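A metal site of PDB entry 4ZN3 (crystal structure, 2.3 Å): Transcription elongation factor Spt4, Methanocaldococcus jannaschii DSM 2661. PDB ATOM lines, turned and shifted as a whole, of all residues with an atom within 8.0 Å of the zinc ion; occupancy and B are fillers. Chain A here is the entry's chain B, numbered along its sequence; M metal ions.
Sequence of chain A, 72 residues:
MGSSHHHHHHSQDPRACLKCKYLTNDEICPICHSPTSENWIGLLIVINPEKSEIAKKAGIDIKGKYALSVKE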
ATOM      1  N   ALA A  16     -11.037 -18.802  20.486  1.00  0.00           N
ATOM      2  CA  ALA A  16     -10.881 -20.016  21.295  1.00  0.00           C
ATOM      3  C   ALA A  16     -11.761 -19.987  22.545  1.00  0.00           C
ATOM      4  O   ALA A  16     -11.788 -18.989  23.252  1.00  0.00           O
ATOM      5  CB  ALA A  16      -9.424 -20.204  21.682  1.00  0.00           C
ATOM      6  N   CYS A  17     -12.470 -21.102  22.798  1.00  0.00           N
ATOM      7  CA  CYS A  17     -13.306 -21.262  23.999  1.00  0.00           C
ATOM      8  C   CYS A  17     -12.481 -21.079  25.260  1.00  0.00           C
ATOM      9  O   CYS A  17     -11.422 -21.708  25.407  1.00  0.00           O
ATOM     10  CB  CYS A  17     -13.929 -22.657  24.037  1.00  0.00           C
ATOM     11  SG  CYS A  17     -14.885 -23.012  25.518  1.00  0.00           S
ATOM     12  N   LEU A  18     -12.943 -20.223  26.170  1.00  0.00           N
ATOM     13  CA  LEU A  18     -12.198 -19.963  27.416  1.00  0.00           C
ATOM     14  C   LEU A  18     -12.163 -21.192  28.345  1.00  0.00           C
ATOM     15  O   LEU A  18     -11.190 -21.381  29.077  1.00  0.00           O
ATOM     16  CB  LEU A  18     -12.741 -18.732  28.145  1.00  0.00           C
ATOM     17  CG  LEU A  18     -12.357 -17.392  27.515  1.00  0.00           C
ATOM     18  CD1 LEU A  18     -13.291 -16.290  27.996  1.00  0.00           C
ATOM     19  CD2 LEU A  18     -10.911 -17.036  27.823  1.00  0.00           C
ATOM     20  N   LYS A  19     -13.196 -22.024  28.308  1.00  0.00           N
ATOM     21  CA  LYS A  19     -13.262 -23.207  29.163  1.00  0.00           C
ATOM     22  C   LYS A  19     -12.472 -24.386  28.574  1.00  0.00           C
ATOM     23  O   LYS A  19     -11.566 -24.900  29.234  1.00  0.00           O
ATOM     24  CB  LYS A  19     -14.720 -23.608  29.428  1.00  0.00           C
ATOM     25  CG  LYS A  19     -14.974 -24.060  30.852  1.00  0.00           C
ATOM     26  CD  LYS A  19     -16.351 -24.692  31.031  1.00  0.00           C
ATOM     27  CE  LYS A  19     -16.399 -26.138  30.558  1.00  0.00           C
ATOM     28  NZ  LYS A  19     -17.356 -26.958  31.363  1.00  0.00           N
ATOM     29  N   CYS A  20     -12.788 -24.781  27.340  1.00  0.00           N
ATOM     30  CA  CYS A  20     -12.228 -26.000  26.732  1.00  0.00           C
ATOM     31  C   CYS A  20     -11.242 -25.785  25.570  1.00  0.00           C
ATOM     32  O   CYS A  20     -10.743 -26.766  25.028  1.00  0.00           O
ATOM     33  CB  CYS A  20     -13.363 -26.914  26.268  1.00  0.00           C
ATOM     34  SG  CYS A  20     -14.096 -26.489  24.674  1.00  0.00           S
ATOM     35  N   LYS A  21     -10.986 -24.529  25.184  1.00  0.00           N
ATOM     36  CA  LYS A  21      -9.981 -24.151  24.163  1.00  0.00           C
ATOM     37  C   LYS A  21     -10.308 -24.490  22.686  1.00  0.00           C
ATOM     38  O   LYS A  21      -9.507 -24.196  21.797  1.00  0.00           O
ATOM     39  CB  LYS A  21      -8.567 -24.640  24.556  1.00  0.00           C
ATOM     40  CG  LYS A  21      -8.063 -23.995  25.839  1.00  0.00           C
ATOM     41  CD  LYS A  21      -6.761 -24.614  26.318  1.00  0.00           C
ATOM     42  CE  LYS A  21      -6.985 -25.924  27.058  1.00  0.00           C
ATOM     43  NZ  LYS A  21      -5.749 -26.351  27.766  1.00  0.00           N
ATOM     44  N   TYR A  22     -11.496 -25.037  22.441  1.00  0.00           N
ATOM     45  CA  TYR A  22     -11.963 -25.396  21.103  1.00  0.00           C
ATOM     46  C   TYR A  22     -12.002 -24.156  20.205  1.00  0.00           C
ATOM     47  O   TYR A  22     -12.494 -23.107  20.603  1.00  0.00           O
ATOM     48  CB  TYR A  22     -13.356 -26.016  21.221  1.00  0.00           C
ATOM     49  CG  TYR A  22     -13.970 -26.529  19.940  1.00  0.00           C
ATOM     50  CD1 TYR A  22     -13.701 -27.819  19.493  1.00  0.00           C
ATOM     51  CD2 TYR A  22     -14.844 -25.744  19.187  1.00  0.00           C
ATOM     52  CE1 TYR A  22     -14.260 -28.306  18.331  1.00  0.00           C
ATOM     53  CE2 TYR A  22     -15.406 -26.222  18.015  1.00  0.00           C
ATOM     54  CZ  TYR A  22     -15.119 -27.504  17.597  1.00  0.00           C
ATOM     55  OH  TYR A  22     -15.665 -27.996  16.445  1.00  0.00           O
ATOM     56  N   LEU A  23     -11.475 -24.297  18.986  1.00  0.00           N
ATOM     57  CA  LEU A  23     -11.429 -23.179  18.035  1.00  0.00           C
ATOM     58  C   LEU A  23     -12.739 -23.026  17.271  1.00  0.00           C
ATOM     59  O   LEU A  23     -13.348 -24.017  16.857  1.00  0.00           O
ATOM     60  CB  LEU A  23     -10.258 -23.335  17.055  1.00  0.00           C
ATOM     61  CG  LEU A  23      -8.841 -23.376  17.644  1.00  0.00           C
ATOM     62  CD1 LEU A  23      -7.804 -23.395  16.535  1.00  0.00           C
ATOM     63  CD2 LEU A  23      -8.553 -22.211  18.596  1.00  0.00           C
ATOM     64  N   THR A  24     -13.165 -21.785  17.088  1.00  0.00           N
ATOM     65  CA  THR A  24     -14.403 -21.443  16.385  1.00  0.00           C
ATOM     66  C   THR A  24     -14.452 -19.951  16.053  1.00  0.00           C
ATOM     67  O   THR A  24     -13.804 -19.154  16.728  1.00  0.00           O
ATOM     68  CB  THR A  24     -15.636 -21.805  17.242  1.00  0.00           C
ATOM     69  OG1 THR A  24     -16.829 -21.349  16.582  1.00  0.00           O
ATOM     70  CG2 THR A  24     -15.554 -21.164  18.640  1.00  0.00           C
ATOM     71  N   ILE A  28     -19.509 -17.625  21.238  1.00  0.00           N
ATOM     72  CA  ILE A  28     -19.633 -18.637  22.283  1.00  0.00           C
ATOM     73  C   ILE A  28     -19.283 -20.013  21.700  1.00  0.00           C
ATOM     74  O   ILE A  28     -19.497 -20.274  20.510  1.00  0.00           O
ATOM     75  CB  ILE A  28     -21.032 -18.622  22.947  1.00  0.00           C
ATOM     76  CG1 ILE A  28     -22.137 -19.150  22.012  1.00  0.00           C
ATOM     77  CG2 ILE A  28     -21.382 -17.220  23.438  1.00  0.00           C
ATOM     78  CD1 ILE A  28     -22.518 -20.595  22.276  1.00  0.00           C
ATOM     79  N   CYS A  29     -18.750 -20.879  22.564  1.00  0.00           N
ATOM     80  CA  CYS A  29     -18.272 -22.190  22.150  1.00  0.00           C
ATOM     81  C   CYS A  29     -19.414 -23.113  21.737  1.00  0.00           C
ATOM     82  O   CYS A  29     -20.329 -23.326  22.519  1.00  0.00           O
ATOM     83  CB  CYS A  29     -17.518 -22.834  23.315  1.00  0.00           C
ATOM     84  SG  CYS A  29     -16.878 -24.486  22.971  1.00  0.00           S
ATOM     85  N   PRO A  30     -19.351 -23.682  20.516  1.00  0.00           N
ATOM     86  CA  PRO A  30     -20.403 -24.648  20.126  1.00  0.00           C
ATOM     87  C   PRO A  30     -20.440 -25.916  20.986  1.00  0.00           C
ATOM     88  O   PRO A  30     -21.496 -26.558  21.068  1.00  0.00           O
ATOM     89  CB  PRO A  30     -20.066 -25.007  18.667  1.00  0.00           C
ATOM     90  CG  PRO A  30     -18.950 -24.119  18.251  1.00  0.00           C
ATOM     91  CD  PRO A  30     -18.307 -23.568  19.480  1.00  0.00           C
ATOM     92  N   ILE A  31     -19.324 -26.274  21.608  1.00  0.00           N
ATOM     93  CA  ILE A  31     -19.238 -27.469  22.435  1.00  0.00           C
ATOM     94  C   ILE A  31     -19.838 -27.207  23.817  1.00  0.00           C
ATOM     95  O   ILE A  31     -20.845 -27.805  24.168  1.00  0.00           O
ATOM     96  CB  ILE A  31     -17.779 -28.000  22.561  1.00  0.00           C
ATOM     97  CG1 ILE A  31     -17.129 -28.192  21.177  1.00  0.00           C
ATOM     98  CG2 ILE A  31     -17.741 -29.299  23.363  1.00  0.00           C
ATOM     99  CD1 ILE A  31     -17.902 -29.062  20.203  1.00  0.00           C
ATOM    100  N   CYS A  32     -19.212 -26.316  24.587  1.00  0.00           N
ATOM    101  CA  CYS A  32     -19.585 -26.099  26.003  1.00  0.00           C
ATOM    102  C   CYS A  32     -20.311 -24.776  26.303  1.00  0.00           C
ATOM    103  O   CYS A  32     -20.641 -24.506  27.457  1.00  0.00           O
ATOM    104  CB  CYS A  32     -18.349 -26.219  26.885  1.00  0.00           C
ATOM    105  SG  CYS A  32     -17.268 -24.767  26.888  1.00  0.00           S
ATOM    106  N   HIS A  33     -20.516 -23.942  25.274  1.00  0.00           N
ATOM    107  CA  HIS A  33     -21.312 -22.698  25.378  1.00  0.00           C
ATOM    108  C   HIS A  33     -20.716 -21.567  26.245  1.00  0.00           C
ATOM    109  O   HIS A  33     -21.405 -20.593  26.535  1.00  0.00           O
ATOM    110  CB  HIS A  33     -22.767 -22.983  25.788  1.00  0.00           C
ATOM    111  CG  HIS A  33     -23.443 -24.003  24.914  1.00  0.00           C
ATOM    112  ND1 HIS A  33     -23.859 -25.226  25.386  1.00  0.00           N
ATOM    113  CD2 HIS A  33     -23.759 -23.979  23.597  1.00  0.00           C
ATOM    114  CE1 HIS A  33     -24.423 -25.906  24.395  1.00  0.00           C
ATOM    115  NE2 HIS A  33     -24.360 -25.173  23.304  1.00  0.00           N
ATOM    116  N   SER A  34     -19.444 -21.681  26.646  1.00  0.00           N
ATOM    117  CA  SER A  34     -18.795 -20.584  27.365  1.00  0.00           C
ATOM    118  C   SER A  34     -18.355 -19.533  26.352  1.00  0.00           C
ATOM    119  O   SER A  34     -18.338 -19.820  25.146  1.00  0.00           O
ATOM    120  CB  SER A  34     -17.626 -21.090  28.207  1.00  0.00           C
ATOM    121  OG  SER A  34     -16.445 -21.240  27.437  1.00  0.00           O
ATOM    122  N   PRO A  35     -17.994 -18.318  26.811  1.00  0.00           N
ATOM    123  CA  PRO A  35     -17.484 -17.313  25.871  1.00  0.00           C
ATOM    124  C   PRO A  35     -16.177 -17.731  25.217  1.00  0.00           C
ATOM    125  O   PRO A  35     -15.387 -18.458  25.826  1.00  0.00           O
ATOM    126  CB  PRO A  35     -17.257 -16.068  26.747  1.00  0.00           C
ATOM    127  CG  PRO A  35     -18.048 -16.294  27.982  1.00  0.00           C
ATOM    128  CD  PRO A  35     -18.099 -17.776  28.182  1.00  0.00           C
ATOM    129  N   THR A  36     -15.963 -17.281  23.983  1.00  0.00           N
ATOM    130  CA  THR A  36     -14.706 -17.465  23.276  1.00  0.00           C
ATOM    131  C   THR A  36     -13.883 -16.212  23.428  1.00  0.00           C
ATOM    132  O   THR A  36     -14.385 -15.166  23.826  1.00  0.00           O
ATOM    133  CB  THR A  36     -14.910 -17.762  21.778  1.00  0.00           C
ATOM    134  OG1 THR A  36     -15.519 -16.644  21.129  1.00  0.00           O
ATOM    135  CG2 THR A  36     -15.761 -18.995  21.585  1.00  0.00           C
ATOM    136  N   TYR A  66      -7.821 -27.107  18.689  1.00  0.00           N
ATOM    137  CA  TYR A  66      -7.760 -26.468  19.997  1.00  0.00           C
ATOM    138  C   TYR A  66      -6.564 -25.554  20.112  1.00  0.00           C
ATOM    139  O   TYR A  66      -5.504 -25.840  19.558  1.00  0.00           O
ATOM    140  CB  TYR A  66      -7.634 -27.528  21.088  1.00  0.00           C
ATOM    141  CG  TYR A  66      -8.836 -28.420  21.233  1.00  0.00           C
ATOM    142  CD1 TYR A  66      -9.034 -29.505  20.378  1.00  0.00           C
ATOM    143  CD2 TYR A  66      -9.770 -28.180  22.231  1.00  0.00           C
ATOM    144  CE1 TYR A  66     -10.133 -30.328  20.520  1.00  0.00           C
ATOM    145  CE2 TYR A  66     -10.882 -28.997  22.373  1.00  0.00           C
ATOM    146  CZ  TYR A  66     -11.064 -30.066  21.517  1.00  0.00           C
ATOM    147  OH  TYR A  66     -12.160 -30.867  21.668  1.00  0.00           O
HETATM  148 ZN    ZN M   1     -15.792 -24.849  24.966  1.00  0.00          ZN
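The side-chain sulfur (SG) of Cys 17 lies close to the side-chain hydroxyl (OG) of Ser 34, at 3.0 Å.
The backbone carbonyl oxygen (O) of Tyr 22 lies within hydrogen-bond range of the backbone NH (N) of Cys 17 (3.0 Å).
N of Lys 19 lies close to SG of Cys 17, at 3.4 Å.
The backbone carbonyl oxygen (O) of Ser 34 lies within hydrogen-bond range of the backbone NH (N) of Cys 29, at 2.8 Å.
The side-chain sulfur (SG) of Cys 29 sits close to the backbone NH (N) of Ile 31.
SG of Cys 20 sits close to N of Tyr 22, at 3.7 Å.
The side-chain sulfur (SG) of Cys 32 sits close to the side-chain hydroxyl (OG) of Ser 34 (3.7 Å).
The nearest printed residue that does not touch the zinc ion is Ser 34 (4.4 Å).
The zinc ion is bound by SG of Cys 17 (2.1 Å).
The side-chain sulfur (SG) of Cys 29 is bound to the zinc ion (2.3 Å).
The zinc ion is bound by the side-chain sulfur (SG) of Cys 20 (2.4 Å).
The zinc ion is bound by SG of Cys 32, at 2.4 Å.
The zinc ion has four donor atoms within binding distance.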
